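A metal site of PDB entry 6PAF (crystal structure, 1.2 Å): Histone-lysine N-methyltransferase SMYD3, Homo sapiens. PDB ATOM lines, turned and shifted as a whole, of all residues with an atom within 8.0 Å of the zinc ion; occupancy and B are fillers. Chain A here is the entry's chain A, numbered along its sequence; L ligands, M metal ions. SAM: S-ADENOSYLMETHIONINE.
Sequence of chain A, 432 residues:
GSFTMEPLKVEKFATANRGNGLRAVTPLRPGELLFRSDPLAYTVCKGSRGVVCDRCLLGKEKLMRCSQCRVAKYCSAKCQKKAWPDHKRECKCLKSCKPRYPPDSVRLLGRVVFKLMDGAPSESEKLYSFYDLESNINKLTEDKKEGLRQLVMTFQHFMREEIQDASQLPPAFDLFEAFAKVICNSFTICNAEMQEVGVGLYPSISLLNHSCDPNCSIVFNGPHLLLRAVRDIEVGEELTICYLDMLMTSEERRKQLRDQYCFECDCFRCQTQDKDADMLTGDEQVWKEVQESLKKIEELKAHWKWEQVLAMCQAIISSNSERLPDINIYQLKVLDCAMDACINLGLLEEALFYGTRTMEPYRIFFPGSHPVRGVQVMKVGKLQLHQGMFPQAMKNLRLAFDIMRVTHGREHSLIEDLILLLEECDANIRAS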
ATOM      1  N   HIS A 210       1.094   5.574  -1.014  1.00  0.00           N
ATOM      2  CA  HIS A 210       0.350   6.689  -0.451  1.00  0.00           C
ATOM      3  C   HIS A 210      -0.594   6.235   0.648  1.00  0.00           C
ATOM      4  O   HIS A 210      -1.233   5.169   0.540  1.00  0.00           O
ATOM      5  CB  HIS A 210      -0.510   7.291  -1.561  1.00  0.00           C
ATOM      6  CG  HIS A 210      -1.560   8.225  -1.044  1.00  0.00           C
ATOM      7  ND1 HIS A 210      -1.311   9.554  -0.752  1.00  0.00           N
ATOM      8  CD2 HIS A 210      -2.852   7.984  -0.723  1.00  0.00           C
ATOM      9  CE1 HIS A 210      -2.414  10.090  -0.270  1.00  0.00           C
ATOM     10  NE2 HIS A 210      -3.358   9.152  -0.231  1.00  0.00           N
ATOM     11  N   SER A 211      -0.748   7.074   1.647  1.00  0.00           N
ATOM     12  CA  SER A 211      -1.855   6.975   2.570  1.00  0.00           C
ATOM     13  C   SER A 211      -2.351   8.357   2.902  1.00  0.00           C
ATOM     14  O   SER A 211      -1.569   9.284   3.018  1.00  0.00           O
ATOM     15  CB  SER A 211      -1.452   6.253   3.859  1.00  0.00           C
ATOM     16  OG  SER A 211      -2.499   6.366   4.796  1.00  0.00           O
ATOM     17  N   CYS A 212      -3.663   8.492   3.109  1.00  0.00           N
ATOM     18  CA  CYS A 212      -4.232   9.750   3.591  1.00  0.00           C
ATOM     19  C   CYS A 212      -4.067   9.906   5.089  1.00  0.00           C
ATOM     20  O   CYS A 212      -4.476  10.941   5.617  1.00  0.00           O
ATOM     21  CB  CYS A 212      -5.716   9.922   3.180  1.00  0.00           C
ATOM     22  SG  CYS A 212      -6.105   9.507   1.503  1.00  0.00           S
ATOM     23  N   ASP A 213      -3.490   8.921   5.742  1.00  0.00           N
ATOM     24  CA  ASP A 213      -3.118   9.001   7.148  1.00  0.00           C
ATOM     25  C   ASP A 213      -1.818   8.215   7.306  1.00  0.00           C
ATOM     26  O   ASP A 213      -1.819   7.091   7.800  1.00  0.00           O
ATOM     27  CB  ASP A 213      -4.215   8.397   8.006  1.00  0.00           C
ATOM     28  CG  ASP A 213      -3.874   8.419   9.462  1.00  0.00           C
ATOM     29  OD1 ASP A 213      -2.951   9.139   9.885  1.00  0.00           O
ATOM     30  OD2 ASP A 213      -4.554   7.676  10.188  1.00  0.00           O
ATOM     31  N   CYS A 242       1.857  10.680   2.543  1.00  0.00           N
ATOM     32  CA  CYS A 242       0.703  11.242   1.866  1.00  0.00           C
ATOM     33  C   CYS A 242       1.182  12.032   0.661  1.00  0.00           C
ATOM     34  O   CYS A 242       1.964  12.982   0.784  1.00  0.00           O
ATOM     35  CB  CYS A 242      -0.082  12.129   2.824  1.00  0.00           C
ATOM     36  SG  CYS A 242      -1.608  12.726   2.095  1.00  0.00           S
ATOM     37  N   LEU A 244      -0.439  14.023  -1.056  1.00  0.00           N
ATOM     38  CA  LEU A 244      -1.330  15.139  -1.318  1.00  0.00           C
ATOM     39  C   LEU A 244      -1.306  16.136  -0.168  1.00  0.00           C
ATOM     40  O   LEU A 244      -1.046  15.801   0.981  1.00  0.00           O
ATOM     41  CB  LEU A 244      -2.772  14.620  -1.420  1.00  0.00           C
ATOM     42  CG  LEU A 244      -2.965  13.583  -2.522  1.00  0.00           C
ATOM     43  CD1 LEU A 244      -4.425  13.227  -2.583  1.00  0.00           C
ATOM     44  CD2 LEU A 244      -2.504  14.090  -3.859  1.00  0.00           C
ATOM     45  N   SER A 250     -12.205  14.223   0.516  1.00  0.00           N
ATOM     46  CA  SER A 250     -12.026  12.882  -0.050  1.00  0.00           C
ATOM     47  C   SER A 250     -12.351  12.854  -1.530  1.00  0.00           C
ATOM     48  O   SER A 250     -11.723  12.101  -2.284  1.00  0.00           O
ATOM     49  CB  SER A 250     -12.826  11.829   0.712  1.00  0.00           C
ATOM     50  OG  SER A 250     -14.213  12.064   0.607  1.00  0.00           O
ATOM     51  N   ARG A 253      -9.289  14.330  -3.203  1.00  0.00           N
ATOM     52  CA  ARG A 253      -8.234  13.331  -3.218  1.00  0.00           C
ATOM     53  C   ARG A 253      -8.526  12.264  -4.240  1.00  0.00           C
ATOM     54  O   ARG A 253      -7.626  11.808  -4.955  1.00  0.00           O
ATOM     55  CB  ARG A 253      -8.038  12.708  -1.829  1.00  0.00           C
ATOM     56  CG  ARG A 253      -7.673  13.756  -0.767  1.00  0.00           C
ATOM     57  CD  ARG A 253      -7.064  13.116   0.484  1.00  0.00           C
ATOM     58  NE  ARG A 253      -7.912  12.113   1.123  1.00  0.00           N
ATOM     59  CZ  ARG A 253      -8.944  12.389   1.941  1.00  0.00           C
ATOM     60  NH1 ARG A 253      -9.259  13.639   2.256  1.00  0.00           N
ATOM     61  NH2 ARG A 253      -9.615  11.401   2.461  1.00  0.00           N
ATOM     62  N   ARG A 254      -9.782  11.818  -4.304  1.00  0.00           N
ATOM     63  CA  ARG A 254     -10.111  10.764  -5.265  1.00  0.00           C
ATOM     64  C   ARG A 254      -9.749  11.200  -6.670  1.00  0.00           C
ATOM     65  O   ARG A 254      -9.198  10.432  -7.449  1.00  0.00           O
ATOM     66  CB  ARG A 254     -11.597  10.413  -5.170  1.00  0.00           C
ATOM     67  CG  ARG A 254     -12.081   9.469  -6.267  1.00  0.00           C
ATOM     68  CD  ARG A 254     -13.506   9.004  -6.067  1.00  0.00           C
ATOM     69  NE  ARG A 254     -13.650   8.257  -4.841  1.00  0.00           N
ATOM     70  CZ  ARG A 254     -14.217   8.685  -3.737  1.00  0.00           C
ATOM     71  NH1 ARG A 254     -14.825   9.854  -3.668  1.00  0.00           N
ATOM     72  NH2 ARG A 254     -14.173   7.875  -2.663  1.00  0.00           N
ATOM     73  N   LEU A 257      -5.846  11.312  -7.061  1.00  0.00           N
ATOM     74  CA  LEU A 257      -5.236   9.990  -7.036  1.00  0.00           C
ATOM     75  C   LEU A 257      -5.612   9.200  -8.288  1.00  0.00           C
ATOM     76  O   LEU A 257      -4.787   8.408  -8.788  1.00  0.00           O
ATOM     77  CB  LEU A 257      -5.593   9.254  -5.755  1.00  0.00           C
ATOM     78  CG  LEU A 257      -5.086   9.929  -4.486  1.00  0.00           C
ATOM     79  CD1 LEU A 257      -5.604   9.171  -3.287  1.00  0.00           C
ATOM     80  CD2 LEU A 257      -3.568  10.078  -4.452  1.00  0.00           C
ATOM     81  N   PHE A 263      -5.060   5.218  -9.028  1.00  0.00           N
ATOM     82  CA  PHE A 263      -5.553   4.267  -8.055  1.00  0.00           C
ATOM     83  C   PHE A 263      -6.707   4.877  -7.287  1.00  0.00           C
ATOM     84  O   PHE A 263      -6.896   6.096  -7.280  1.00  0.00           O
ATOM     85  CB  PHE A 263      -4.461   3.697  -7.114  1.00  0.00           C
ATOM     86  CG  PHE A 263      -3.973   4.656  -6.068  1.00  0.00           C
ATOM     87  CD1 PHE A 263      -2.975   5.529  -6.348  1.00  0.00           C
ATOM     88  CD2 PHE A 263      -4.545   4.674  -4.805  1.00  0.00           C
ATOM     89  CE1 PHE A 263      -2.503   6.399  -5.357  1.00  0.00           C
ATOM     90  CE2 PHE A 263      -4.115   5.543  -3.806  1.00  0.00           C
ATOM     91  CZ  PHE A 263      -3.127   6.409  -4.104  1.00  0.00           C
ATOM     92  N   GLU A 264      -7.481   3.982  -6.655  1.00  0.00           N
ATOM     93  CA  GLU A 264      -8.646   4.259  -5.814  1.00  0.00           C
ATOM     94  C   GLU A 264      -8.179   3.985  -4.390  1.00  0.00           C
ATOM     95  O   GLU A 264      -7.634   2.902  -4.117  1.00  0.00           O
ATOM     96  CB  GLU A 264      -9.782   3.267  -6.189  1.00  0.00           C
ATOM     97  CG  GLU A 264      -9.940   2.977  -7.710  1.00  0.00           C
ATOM     98  CD  GLU A 264     -10.385   4.224  -8.453  1.00  0.00           C
ATOM     99  OE1 GLU A 264     -10.403   4.252  -9.698  1.00  0.00           O
ATOM    100  OE2 GLU A 264     -10.748   5.215  -7.782  1.00  0.00           O
ATOM    101  N   CYS A 265      -8.305   4.970  -3.513  1.00  0.00           N
ATOM    102  CA  CYS A 265      -7.696   4.877  -2.180  1.00  0.00           C
ATOM    103  C   CYS A 265      -8.673   4.199  -1.272  1.00  0.00           C
ATOM    104  O   CYS A 265      -9.835   4.613  -1.173  1.00  0.00           O
ATOM    105  CB  CYS A 265      -7.357   6.218  -1.553  1.00  0.00           C
ATOM    106  SG  CYS A 265      -6.348   6.150   0.010  1.00  0.00           S
ATOM    107  N   ASP A 266      -8.159   3.155  -0.586  1.00  0.00           N
ATOM    108  CA  ASP A 266      -8.912   2.330   0.334  1.00  0.00           C
ATOM    109  C   ASP A 266      -8.680   2.702   1.803  1.00  0.00           C
ATOM    110  O   ASP A 266      -9.076   1.936   2.677  1.00  0.00           O
ATOM    111  CB  ASP A 266      -8.654   0.810   0.090  1.00  0.00           C
ATOM    112  CG  ASP A 266      -7.224   0.357   0.477  1.00  0.00           C
ATOM    113  OD1 ASP A 266      -6.366   1.154   0.876  1.00  0.00           O
ATOM    114  OD2 ASP A 266      -6.952  -0.856   0.386  1.00  0.00           O
ATOM    115  N   CYS A 267      -8.020   3.822   2.097  1.00  0.00           N
ATOM    116  CA  CYS A 267      -7.779   4.191   3.502  1.00  0.00           C
ATOM    117  C   CYS A 267      -9.111   4.464   4.273  1.00  0.00           C
ATOM    118  O   CYS A 267     -10.186   4.698   3.712  1.00  0.00           O
ATOM    119  CB  CYS A 267      -6.666   5.229   3.599  1.00  0.00           C
ATOM    120  SG  CYS A 267      -7.413   6.820   3.513  1.00  0.00           S
ATOM    121  N   PHE A 268      -9.072   4.365   5.608  1.00  0.00           N
ATOM    122  CA  PHE A 268     -10.295   4.586   6.401  1.00  0.00           C
ATOM    123  C   PHE A 268     -10.867   6.000   6.193  1.00  0.00           C
ATOM    124  O   PHE A 268     -12.068   6.202   6.210  1.00  0.00           O
ATOM    125  CB  PHE A 268      -9.976   4.430   7.900  1.00  0.00           C
ATOM    126  CG  PHE A 268     -10.984   5.077   8.857  1.00  0.00           C
ATOM    127  CD1 PHE A 268     -12.139   4.405   9.251  1.00  0.00           C
ATOM    128  CD2 PHE A 268     -10.743   6.351   9.349  1.00  0.00           C
ATOM    129  CE1 PHE A 268     -13.032   4.973  10.122  1.00  0.00           C
ATOM    130  CE2 PHE A 268     -11.657   6.929  10.228  1.00  0.00           C
ATOM    131  CZ  PHE A 268     -12.800   6.228  10.604  1.00  0.00           C
ATOM    132  N   ARG A 269      -9.996   6.940   5.973  1.00  0.00           N
ATOM    133  CA  ARG A 269     -10.448   8.313   5.775  1.00  0.00           C
ATOM    134  C   ARG A 269     -11.282   8.423   4.509  1.00  0.00           C
ATOM    135  O   ARG A 269     -12.294   9.100   4.502  1.00  0.00           O
ATOM    136  CB  ARG A 269      -9.275   9.271   5.693  1.00  0.00           C
ATOM    137  CG  ARG A 269      -8.503   9.350   7.000  1.00  0.00           C
ATOM    138  CD  ARG A 269      -7.568  10.533   6.989  1.00  0.00           C
ATOM    139  NE  ARG A 269      -8.359  11.764   6.913  1.00  0.00           N
ATOM    140  CZ  ARG A 269      -8.110  12.776   6.103  1.00  0.00           C
ATOM    141  NH1 ARG A 269      -6.983  12.837   5.374  1.00  0.00           N
ATOM    142  NH2 ARG A 269      -8.965  13.802   6.034  1.00  0.00           N
ATOM    143  N   CYS A 270     -10.874   7.736   3.434  1.00  0.00           N
ATOM    144  CA  CYS A 270     -11.639   7.826   2.184  1.00  0.00           C
ATOM    145  C   CYS A 270     -12.961   7.085   2.315  1.00  0.00           C
ATOM    146  O   CYS A 270     -14.007   7.610   1.905  1.00  0.00           O
ATOM    147  CB  CYS A 270     -10.817   7.331   1.011  1.00  0.00           C
ATOM    148  SG  CYS A 270      -9.442   8.472   0.707  1.00  0.00           S
ATOM    149  N   GLN A 271     -12.967   5.952   3.023  1.00  0.00           N
ATOM    150  CA  GLN A 271     -14.217   5.226   3.193  1.00  0.00           C
ATOM    151  C   GLN A 271     -15.237   6.004   3.971  1.00  0.00           C
ATOM    152  O   GLN A 271     -16.435   5.816   3.807  1.00  0.00           O
ATOM    153  CB  GLN A 271     -13.949   3.944   3.945  1.00  0.00           C
ATOM    154  CG  GLN A 271     -13.845   2.845   3.019  1.00  0.00           C
ATOM    155  CD  GLN A 271     -14.164   1.543   3.724  1.00  0.00           C
ATOM    156  OE1 GLN A 271     -13.273   0.915   4.308  1.00  0.00           O
ATOM    157  NE2 GLN A 271     -15.455   1.186   3.750  1.00  0.00           N
HETATM  158  N   SAM L   1       3.717   0.998  -5.937  1.00  0.00           N
HETATM  159  CA  SAM L   1       4.721   1.818  -6.654  1.00  0.00           C
HETATM  160  C   SAM L   1       5.627   0.959  -7.475  1.00  0.00           C
HETATM  161  O   SAM L   1       6.577   1.519  -8.001  1.00  0.00           O
HETATM  162  OXT SAM L   1       5.353  -0.237  -7.585  1.00  0.00           O
HETATM  163  CB  SAM L   1       5.474   2.739  -5.689  1.00  0.00           C
HETATM  164  CG  SAM L   1       4.727   4.041  -5.364  1.00  0.00           C
HETATM  165  SD  SAM L   1       4.736   5.088  -6.883  1.00  0.00           S
HETATM  166  CE  SAM L   1       5.374   6.676  -6.311  1.00  0.00           C
HETATM  167  C5' SAM L   1       2.997   5.591  -7.150  1.00  0.00           C
HETATM  168  C4' SAM L   1       2.105   4.460  -7.625  1.00  0.00           C
HETATM  169  O4' SAM L   1       1.993   3.446  -6.605  1.00  0.00           O
HETATM  170  C3' SAM L   1       0.677   4.941  -7.892  1.00  0.00           C
HETATM  171  O3' SAM L   1       0.619   5.587  -9.131  1.00  0.00           O
HETATM  172  C2' SAM L   1      -0.069   3.620  -7.791  1.00  0.00           C
HETATM  173  O2' SAM L   1       0.201   2.848  -8.955  1.00  0.00           O
HETATM  174  C1' SAM L   1       0.646   2.980  -6.625  1.00  0.00           C
HETATM  175  N9  SAM L   1       0.065   3.386  -5.346  1.00  0.00           N
HETATM  176  C8  SAM L   1       0.591   4.256  -4.404  1.00  0.00           C
HETATM  177  N7  SAM L   1      -0.169   4.294  -3.317  1.00  0.00           N
HETATM  178  C5  SAM L   1      -1.174   3.413  -3.493  1.00  0.00           C
HETATM  179  C6  SAM L   1      -2.242   3.021  -2.706  1.00  0.00           C
HETATM  180  N6  SAM L   1      -2.495   3.479  -1.476  1.00  0.00           N
HETATM  181  N1  SAM L   1      -3.116   2.092  -3.203  1.00  0.00           N
HETATM  182  C2  SAM L   1      -2.915   1.586  -4.449  1.00  0.00           C
HETATM  183  N3  SAM L   1      -1.895   1.928  -5.266  1.00  0.00           N
HETATM  184  C4  SAM L   1      -1.024   2.823  -4.754  1.00  0.00           C
HETATM  185 ZN    ZN M   1      -7.451   7.559   1.436  1.00  0.00          ZN
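The backbone NH (N) of His 210 sits at hydrogen-bond distance from a nitrogen (N7) of the ligand, at 2.9 Å. The backbone carbonyl oxygen (O) of His 210 lies within hydrogen-bond range of a nitrogen (N6) of the ligand (2.9 Å).
The guanidinium group (NE) of Arg 253 lies close to the side-chain sulfur (SG) of Cys 212 (3.2 Å). The side-chain sulfur (SG) of Cys 267 lies close to the backbone NH (N) of Arg 269 (3.6 Å). The backbone carbonyl oxygen (O) of Cys 212 sits at hydrogen-bond distance from the guanidinium group (NH1) of Arg 269 (3.2 Å). The backbone NH of Cys 212 lies within hydrogen-bond range of a ring nitrogen (NE2) of His 210. NH2 of Arg 253 lies close to SG of Cys 270 (3.4 Å).
Four residues have an atom within 4 Å of the zinc ion: Cys 212, Cys 265, Cys 267 and Cys 270. The nearest printed residue that does not touch the zinc ion is Arg 253 (4.5 Å).
The zinc ion is bound by the side-chain sulfur of Cys 267 (2.2 Å), the side-chain sulfur of Cys 265 (2.3 Å), the side-chain sulfur of Cys 270 (2.3 Å) and the side-chain sulfur of Cys 212 (2.4 Å).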
